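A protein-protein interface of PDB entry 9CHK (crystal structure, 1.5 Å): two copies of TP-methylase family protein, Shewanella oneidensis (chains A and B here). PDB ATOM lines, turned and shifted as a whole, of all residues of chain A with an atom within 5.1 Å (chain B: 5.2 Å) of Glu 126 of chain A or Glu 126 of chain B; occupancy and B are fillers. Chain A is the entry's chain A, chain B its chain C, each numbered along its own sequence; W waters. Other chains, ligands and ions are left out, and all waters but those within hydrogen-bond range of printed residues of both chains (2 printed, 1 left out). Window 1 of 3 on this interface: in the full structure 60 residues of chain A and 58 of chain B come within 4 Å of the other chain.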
ATOM      1  N   SER A 124      11.400 -18.408 -26.883  1.00  0.00           N
ATOM      2  CA  SER A 124      12.468 -17.608 -26.299  1.00  0.00           C
ATOM      3  C   SER A 124      13.766 -17.757 -27.092  1.00  0.00           C
ATOM      4  O   SER A 124      13.871 -18.588 -27.993  1.00  0.00           O
ATOM      5  CB  SER A 124      12.700 -17.999 -24.865  1.00  0.00           C
ATOM      6  OG  SER A 124      13.345 -19.266 -24.807  1.00  0.00           O
ATOM      7  N   ALA A 125      14.770 -16.953 -26.721  1.00  0.00           N
ATOM      8  CA  ALA A 125      16.084 -17.024 -27.342  1.00  0.00           C
ATOM      9  C   ALA A 125      16.697 -18.412 -27.179  1.00  0.00           C
ATOM     10  O   ALA A 125      17.383 -18.885 -28.085  1.00  0.00           O
ATOM     11  CB  ALA A 125      16.995 -15.961 -26.761  1.00  0.00           C
ATOM     12  N   GLU A 126      16.464 -19.060 -26.030  1.00  0.00           N
ATOM     13  CA  GLU A 126      17.073 -20.360 -25.788  1.00  0.00           C
ATOM     14  C   GLU A 126      16.367 -21.418 -26.635  1.00  0.00           C
ATOM     15  O   GLU A 126      17.015 -22.320 -27.156  1.00  0.00           O
ATOM     16  CB  GLU A 126      17.200 -20.686 -24.296  1.00  0.00           C
ATOM     17  CG  GLU A 126      15.915 -21.111 -23.594  1.00  0.00           C
ATOM     18  CD  GLU A 126      16.157 -21.534 -22.153  1.00  0.00           C
ATOM     19  OE1 GLU A 126      17.260 -21.257 -21.630  1.00  0.00           O
ATOM     20  OE2 GLU A 126      15.260 -22.161 -21.553  1.00  0.00           O
ATOM     21  N   ALA A 127      15.055 -21.260 -26.838  1.00  0.00           N
ATOM     22  CA  ALA A 127      14.322 -22.143 -27.731  1.00  0.00           C
ATOM     23  C   ALA A 127      14.939 -22.094 -29.132  1.00  0.00           C
ATOM     24  O   ALA A 127      15.091 -23.124 -29.782  1.00  0.00           O
ATOM     25  CB  ALA A 127      12.855 -21.767 -27.750  1.00  0.00           C
ATOM     26  N   CYS A 128      15.295 -20.885 -29.582  1.00  0.00           N
ATOM     27  CA  CYS A 128      15.938 -20.692 -30.871  1.00  0.00           C
ATOM     28  C   CYS A 128      17.335 -21.312 -30.885  1.00  0.00           C
ATOM     29  O   CYS A 128      17.738 -21.905 -31.882  1.00  0.00           O
ATOM     30  CB  CYS A 128      16.008 -19.214 -31.237  1.00  0.00           C
ATOM     31  SG  CYS A 128      14.390 -18.474 -31.566  1.00  0.00           S
ATOM     32  N   LEU A 129      18.068 -21.182 -29.773  1.00  0.00           N
ATOM     33  CA  LEU A 129      19.427 -21.696 -29.693  1.00  0.00           C
ATOM     34  C   LEU A 129      19.430 -23.210 -29.912  1.00  0.00           C
ATOM     35  O   LEU A 129      20.240 -23.723 -30.685  1.00  0.00           O
ATOM     36  CB  LEU A 129      20.022 -21.304 -28.340  1.00  0.00           C
ATOM     37  CG  LEU A 129      21.507 -21.615 -28.114  1.00  0.00           C
ATOM     38  CD1 LEU A 129      22.039 -20.732 -26.995  1.00  0.00           C
ATOM     39  CD2 LEU A 129      21.733 -23.075 -27.782  1.00  0.00           C
ATOM     40  N   TRP A 130      18.542 -23.936 -29.222  1.00  0.00           N
ATOM     41  CA  TRP A 130      18.539 -25.391 -29.339  1.00  0.00           C
ATOM     42  C   TRP A 130      18.372 -25.807 -30.797  1.00  0.00           C
ATOM     43  O   TRP A 130      19.027 -26.737 -31.255  1.00  0.00           O
ATOM     44  CB  TRP A 130      17.439 -26.043 -28.488  1.00  0.00           C
ATOM     45  CG  TRP A 130      17.454 -25.644 -27.039  1.00  0.00           C
ATOM     46  CD1 TRP A 130      16.371 -25.288 -26.291  1.00  0.00           C
ATOM     47  CD2 TRP A 130      18.595 -25.583 -26.155  1.00  0.00           C
ATOM     48  NE1 TRP A 130      16.757 -24.986 -25.015  1.00  0.00           N
ATOM     49  CE2 TRP A 130      18.110 -25.158 -24.900  1.00  0.00           C
ATOM     50  CE3 TRP A 130      19.964 -25.834 -26.301  1.00  0.00           C
ATOM     51  CZ2 TRP A 130      18.950 -24.984 -23.803  1.00  0.00           C
ATOM     52  CZ3 TRP A 130      20.791 -25.664 -25.213  1.00  0.00           C
ATOM     53  CH2 TRP A 130      20.288 -25.242 -23.984  1.00  0.00           C
ATOM     54  N   HIS A 142      20.884 -28.641 -18.876  1.00  0.00           N
ATOM     55  CA  HIS A 142      20.999 -27.241 -19.247  1.00  0.00           C
ATOM     56  C   HIS A 142      20.894 -26.377 -17.993  1.00  0.00           C
ATOM     57  O   HIS A 142      20.135 -26.690 -17.082  1.00  0.00           O
ATOM     58  CB  HIS A 142      19.911 -26.910 -20.274  1.00  0.00           C
ATOM     59  CG  HIS A 142      19.451 -25.494 -20.253  1.00  0.00           C
ATOM     60  ND1 HIS A 142      18.115 -25.163 -20.210  1.00  0.00           N
ATOM     61  CD2 HIS A 142      20.125 -24.338 -20.243  1.00  0.00           C
ATOM     62  CE1 HIS A 142      17.999 -23.842 -20.189  1.00  0.00           C
ATOM     63  NE2 HIS A 142      19.208 -23.322 -20.210  1.00  0.00           N
ATOM     64  N   SER A 144      20.811 -21.993 -16.970  1.00  0.00           N
ATOM     65  CA  SER A 144      20.797 -20.602 -17.398  1.00  0.00           C
ATOM     66  C   SER A 144      20.976 -19.687 -16.191  1.00  0.00           C
ATOM     67  O   SER A 144      20.334 -19.883 -15.164  1.00  0.00           O
ATOM     68  CB  SER A 144      19.516 -20.242 -18.119  1.00  0.00           C
ATOM     69  OG  SER A 144      19.491 -20.716 -19.460  1.00  0.00           O
ATOM     70  N   LEU A 164      24.186 -21.447 -20.204  1.00  0.00           N
ATOM     71  CA  LEU A 164      23.846 -20.215 -20.898  1.00  0.00           C
ATOM     72  C   LEU A 164      24.021 -19.038 -19.946  1.00  0.00           C
ATOM     73  O   LEU A 164      23.432 -19.022 -18.868  1.00  0.00           O
ATOM     74  CB  LEU A 164      22.406 -20.264 -21.409  1.00  0.00           C
ATOM     75  CG  LEU A 164      22.112 -21.213 -22.576  1.00  0.00           C
ATOM     76  CD1 LEU A 164      20.688 -20.980 -23.055  1.00  0.00           C
ATOM     77  CD2 LEU A 164      23.102 -21.039 -23.716  1.00  0.00           C
ATOM     78  N   TRP A 166      23.072 -15.253 -19.960  1.00  0.00           N
ATOM     79  CA  TRP A 166      22.245 -14.263 -20.629  1.00  0.00           C
ATOM     80  C   TRP A 166      22.740 -12.860 -20.288  1.00  0.00           C
ATOM     81  O   TRP A 166      23.345 -12.647 -19.243  1.00  0.00           O
ATOM     82  CB  TRP A 166      20.784 -14.426 -20.193  1.00  0.00           C
ATOM     83  CG  TRP A 166      20.143 -15.743 -20.544  1.00  0.00           C
ATOM     84  CD1 TRP A 166      20.489 -16.981 -20.095  1.00  0.00           C
ATOM     85  CD2 TRP A 166      18.965 -15.929 -21.358  1.00  0.00           C
ATOM     86  NE1 TRP A 166      19.643 -17.929 -20.604  1.00  0.00           N
ATOM     87  CE2 TRP A 166      18.687 -17.313 -21.367  1.00  0.00           C
ATOM     88  CE3 TRP A 166      18.124 -15.068 -22.069  1.00  0.00           C
ATOM     89  CZ2 TRP A 166      17.612 -17.845 -22.072  1.00  0.00           C
ATOM     90  CZ3 TRP A 166      17.061 -15.595 -22.763  1.00  0.00           C
ATOM     91  CH2 TRP A 166      16.799 -16.962 -22.746  1.00  0.00           C
ATOM     92  N   SER B 124       7.832 -25.215 -25.518  1.00  0.00           N
ATOM     93  CA  SER B 124       8.085 -26.435 -24.768  1.00  0.00           C
ATOM     94  C   SER B 124       7.304 -26.430 -23.458  1.00  0.00           C
ATOM     95  O   SER B 124       6.724 -25.419 -23.068  1.00  0.00           O
ATOM     96  CB  SER B 124       9.554 -26.584 -24.485  1.00  0.00           C
ATOM     97  OG  SER B 124       9.964 -25.611 -23.533  1.00  0.00           O
ATOM     98  N   ALA B 125       7.352 -27.564 -22.751  1.00  0.00           N
ATOM     99  CA  ALA B 125       6.697 -27.686 -21.460  1.00  0.00           C
ATOM    100  C   ALA B 125       7.296 -26.693 -20.466  1.00  0.00           C
ATOM    101  O   ALA B 125       6.588 -26.170 -19.612  1.00  0.00           O
ATOM    102  CB  ALA B 125       6.813 -29.108 -20.964  1.00  0.00           C
ATOM    103  N   GLU B 126       8.601 -26.434 -20.596  1.00  0.00           N
ATOM    104  CA  GLU B 126       9.297 -25.508 -19.717  1.00  0.00           C
ATOM    105  C   GLU B 126       8.760 -24.096 -19.946  1.00  0.00           C
ATOM    106  O   GLU B 126       8.508 -23.356 -18.997  1.00  0.00           O
ATOM    107  CB  GLU B 126      10.785 -25.735 -19.985  1.00  0.00           C
ATOM    108  CG  GLU B 126      11.709 -24.629 -19.493  1.00  0.00           C
ATOM    109  CD  GLU B 126      13.161 -24.966 -19.780  1.00  0.00           C
ATOM    110  OE1 GLU B 126      13.626 -26.019 -19.292  1.00  0.00           O
ATOM    111  OE2 GLU B 126      13.824 -24.189 -20.495  1.00  0.00           O
ATOM    112  N   ALA B 127       8.551 -23.744 -21.217  1.00  0.00           N
ATOM    113  CA  ALA B 127       8.003 -22.446 -21.574  1.00  0.00           C
ATOM    114  C   ALA B 127       6.627 -22.263 -20.937  1.00  0.00           C
ATOM    115  O   ALA B 127       6.300 -21.186 -20.442  1.00  0.00           O
ATOM    116  CB  ALA B 127       7.942 -22.314 -23.078  1.00  0.00           C
ATOM    117  N   CYS B 128       5.822 -23.330 -20.947  1.00  0.00           N
ATOM    118  CA  CYS B 128       4.496 -23.292 -20.356  1.00  0.00           C
ATOM    119  C   CYS B 128       4.588 -23.128 -18.841  1.00  0.00           C
ATOM    120  O   CYS B 128       3.784 -22.416 -18.243  1.00  0.00           O
ATOM    121  CB  CYS B 128       3.701 -24.541 -20.714  1.00  0.00           C
ATOM    122  SG  CYS B 128       3.241 -24.623 -22.464  1.00  0.00           S
ATOM    123  N   LEU B 129       5.569 -23.795 -18.224  1.00  0.00           N
ATOM    124  CA  LEU B 129       5.736 -23.749 -16.780  1.00  0.00           C
ATOM    125  C   LEU B 129       6.000 -22.319 -16.307  1.00  0.00           C
ATOM    126  O   LEU B 129       5.389 -21.870 -15.340  1.00  0.00           O
ATOM    127  CB  LEU B 129       6.861 -24.697 -16.369  1.00  0.00           C
ATOM    128  CG  LEU B 129       7.078 -24.884 -14.864  1.00  0.00           C
ATOM    129  CD1 LEU B 129       7.787 -26.202 -14.621  1.00  0.00           C
ATOM    130  CD2 LEU B 129       7.862 -23.739 -14.238  1.00  0.00           C
ATOM    131  N   TRP B 130       6.917 -21.600 -16.968  1.00  0.00           N
ATOM    132  CA  TRP B 130       7.251 -20.250 -16.528  1.00  0.00           C
ATOM    133  C   TRP B 130       5.994 -19.383 -16.524  1.00  0.00           C
ATOM    134  O   TRP B 130       5.785 -18.590 -15.612  1.00  0.00           O
ATOM    135  CB  TRP B 130       8.335 -19.612 -17.407  1.00  0.00           C
ATOM    136  CG  TRP B 130       9.603 -20.413 -17.539  1.00  0.00           C
ATOM    137  CD1 TRP B 130      10.253 -20.680 -18.707  1.00  0.00           C
ATOM    138  CD2 TRP B 130      10.384 -21.035 -16.493  1.00  0.00           C
ATOM    139  NE1 TRP B 130      11.367 -21.434 -18.473  1.00  0.00           N
ATOM    140  CE2 TRP B 130      11.479 -21.664 -17.126  1.00  0.00           C
ATOM    141  CE3 TRP B 130      10.270 -21.130 -15.100  1.00  0.00           C
ATOM    142  CZ2 TRP B 130      12.442 -22.377 -16.415  1.00  0.00           C
ATOM    143  CZ3 TRP B 130      11.232 -21.825 -14.398  1.00  0.00           C
ATOM    144  CH2 TRP B 130      12.299 -22.443 -15.049  1.00  0.00           C
ATOM    145  N   HIS B 142      18.241 -21.194 -13.464  1.00  0.00           N
ATOM    146  CA  HIS B 142      17.443 -22.341 -13.863  1.00  0.00           C
ATOM    147  C   HIS B 142      18.381 -23.480 -14.245  1.00  0.00           C
ATOM    148  O   HIS B 142      19.363 -23.265 -14.952  1.00  0.00           O
ATOM    149  CB  HIS B 142      16.531 -21.947 -15.033  1.00  0.00           C
ATOM    150  CG  HIS B 142      16.028 -23.083 -15.857  1.00  0.00           C
ATOM    151  ND1 HIS B 142      16.058 -23.078 -17.236  1.00  0.00           N
ATOM    152  CD2 HIS B 142      15.500 -24.262 -15.499  1.00  0.00           C
ATOM    153  CE1 HIS B 142      15.561 -24.223 -17.682  1.00  0.00           C
ATOM    154  NE2 HIS B 142      15.210 -24.953 -16.644  1.00  0.00           N
ATOM    155  N   SER B 144      17.901 -27.602 -15.729  1.00  0.00           N
ATOM    156  CA  SER B 144      17.049 -28.680 -16.213  1.00  0.00           C
ATOM    157  C   SER B 144      17.876 -29.948 -16.388  1.00  0.00           C
ATOM    158  O   SER B 144      18.927 -29.912 -17.019  1.00  0.00           O
ATOM    159  CB  SER B 144      16.392 -28.342 -17.537  1.00  0.00           C
ATOM    160  OG  SER B 144      15.164 -27.653 -17.381  1.00  0.00           O
ATOM    161  N   LEU B 164      14.415 -28.149 -12.623  1.00  0.00           N
ATOM    162  CA  LEU B 164      13.406 -28.981 -13.260  1.00  0.00           C
ATOM    163  C   LEU B 164      13.972 -30.377 -13.492  1.00  0.00           C
ATOM    164  O   LEU B 164      15.032 -30.520 -14.097  1.00  0.00           O
ATOM    165  CB  LEU B 164      12.964 -28.364 -14.588  1.00  0.00           C
ATOM    166  CG  LEU B 164      12.281 -26.994 -14.525  1.00  0.00           C
ATOM    167  CD1 LEU B 164      11.808 -26.598 -15.911  1.00  0.00           C
ATOM    168  CD2 LEU B 164      11.126 -26.978 -13.540  1.00  0.00           C
ATOM    169  N   TRP B 166      12.856 -33.481 -15.578  1.00  0.00           N
ATOM    170  CA  TRP B 166      11.977 -33.948 -16.637  1.00  0.00           C
ATOM    171  C   TRP B 166      11.861 -35.469 -16.571  1.00  0.00           C
ATOM    172  O   TRP B 166      12.762 -36.141 -16.072  1.00  0.00           O
ATOM    173  CB  TRP B 166      12.529 -33.524 -18.003  1.00  0.00           C
ATOM    174  CG  TRP B 166      12.644 -32.038 -18.236  1.00  0.00           C
ATOM    175  CD1 TRP B 166      13.431 -31.140 -17.576  1.00  0.00           C
ATOM    176  CD2 TRP B 166      11.990 -31.296 -19.287  1.00  0.00           C
ATOM    177  NE1 TRP B 166      13.282 -29.888 -18.114  1.00  0.00           N
ATOM    178  CE2 TRP B 166      12.417 -29.955 -19.175  1.00  0.00           C
ATOM    179  CE3 TRP B 166      11.094 -31.638 -20.304  1.00  0.00           C
ATOM    180  CZ2 TRP B 166      11.963 -28.963 -20.040  1.00  0.00           C
ATOM    181  CZ3 TRP B 166      10.652 -30.657 -21.161  1.00  0.00           C
ATOM    182  CH2 TRP B 166      11.091 -29.340 -21.035  1.00  0.00           C
HETATM  183  O   HOH W   1      14.561 -25.179 -22.968  1.00  0.00           O
HETATM  184  O   HOH W   2      16.424 -20.795 -19.097  1.00  0.00           O
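Among the printed residues, merely in contact across the chains: His 142 of chain A with His 142 of chain B.
Of chain B, only Glu 126 comes within 4 Å of Glu 126 of chain A. Printed residues of chain A within 4 Å of Glu 126 of chain B: Glu 126 (2.7 Å). Printed residues of chain A within 4 Å of Ser 144 of chain B: His 142 (2.8 Å). Printed residues of chain B within 4 Å of Ser 144 of chain A: His 142. Leu 129 of chain A touches none of the printed residues of chain B. Ala 125 of chain B touches none of the printed residues of chain A. The nearest residue of chain B that does not touch Glu 126 of chain A is His 142 of chain B (4.4 Å). The nearest printed residue of chain A that does not touch Glu 126 of chain B is His 142 of chain A (4.2 Å).
The side-chain carboxylate (OE2) of Glu 126 of chain A sits close to the side-chain carboxylate (OE2) of Glu 126 of chain B (2.7 Å). N of Ser 144 of chain A is in hydrogen-bond range of O of His 142 of chain B, 2.8 Å away. O of His 142 of chain A lies within hydrogen-bond range of N of Ser 144 of chain B.
The indole nitrogen of Trp 130 of chain A lies close to the backbone carbonyl oxygen of Glu 126 of chain A (3.4 Å). The side-chain hydroxyl of Ser 124 of chain A lies close to the backbone NH of Glu 126 of chain A (3.4 Å). NE2 of His 142 of chain B sits at hydrogen-bond distance from OG of Ser 144 of chain B, at 2.8 Å. The indole nitrogen of Trp 130 of chain B lies close to the backbone carbonyl oxygen of Glu 126 of chain B, at 3.5 Å. A ring nitrogen (NE2) of His 142 of chain A sits close to the side-chain carboxylate (OE1) of Glu 126 of chain A, at 3.2 Å. OG of Ser 144 of chain A is in hydrogen-bond range of NE1 of Trp 166 of chain A (3.0 Å).
Printed residues of chain A that touch a printed residue of chain B: Glu 126, His 142 and Ser 144. Hydrophobic or aromatic side chains of chain A within 4 Å of the printed part of chain B: His 142. Of the 11 printed residues of chain B, 3 touch a printed residue of chain A. Hydrophobic or aromatic side chains of chain B that line the printed part of chain A: His 142. Among the printed residues, 4 pairs touch across the chains. Among the printed residues, no Asp or Glu carboxylate lies within 4 Å of a Lys or Arg side-chain nitrogen of the other chain.
Glu 126 of chain B touches its own counterpart, Glu 126 of chain A. His 142 of chain B touches its own counterpart, His 142 of chain A. His 142 of chain A touches Ser 144 of chain B, and with the chains exchanged Ser 144 of chain A touches His 142 of chain B. Positions printed for both chains: 124, 125, 126, 127, 128, 129, 130, 142, 144, 164 and 166.
Water W2 lies within hydrogen-bond range of the side-chain carboxylate (OE1) of Glu 126 of chain A, a ring nitrogen (ND1) of His 142 of chain B and the side-chain hydroxyl (OG) of Ser 144 of chain A. Water W1 lies within hydrogen-bond range of the side-chain carboxylate (OE2) of Glu 126 of chain B, the indole nitrogen (NE1) of Trp 130 of chain A and the side-chain carboxylate (OE2) of Glu 126 of chain A.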
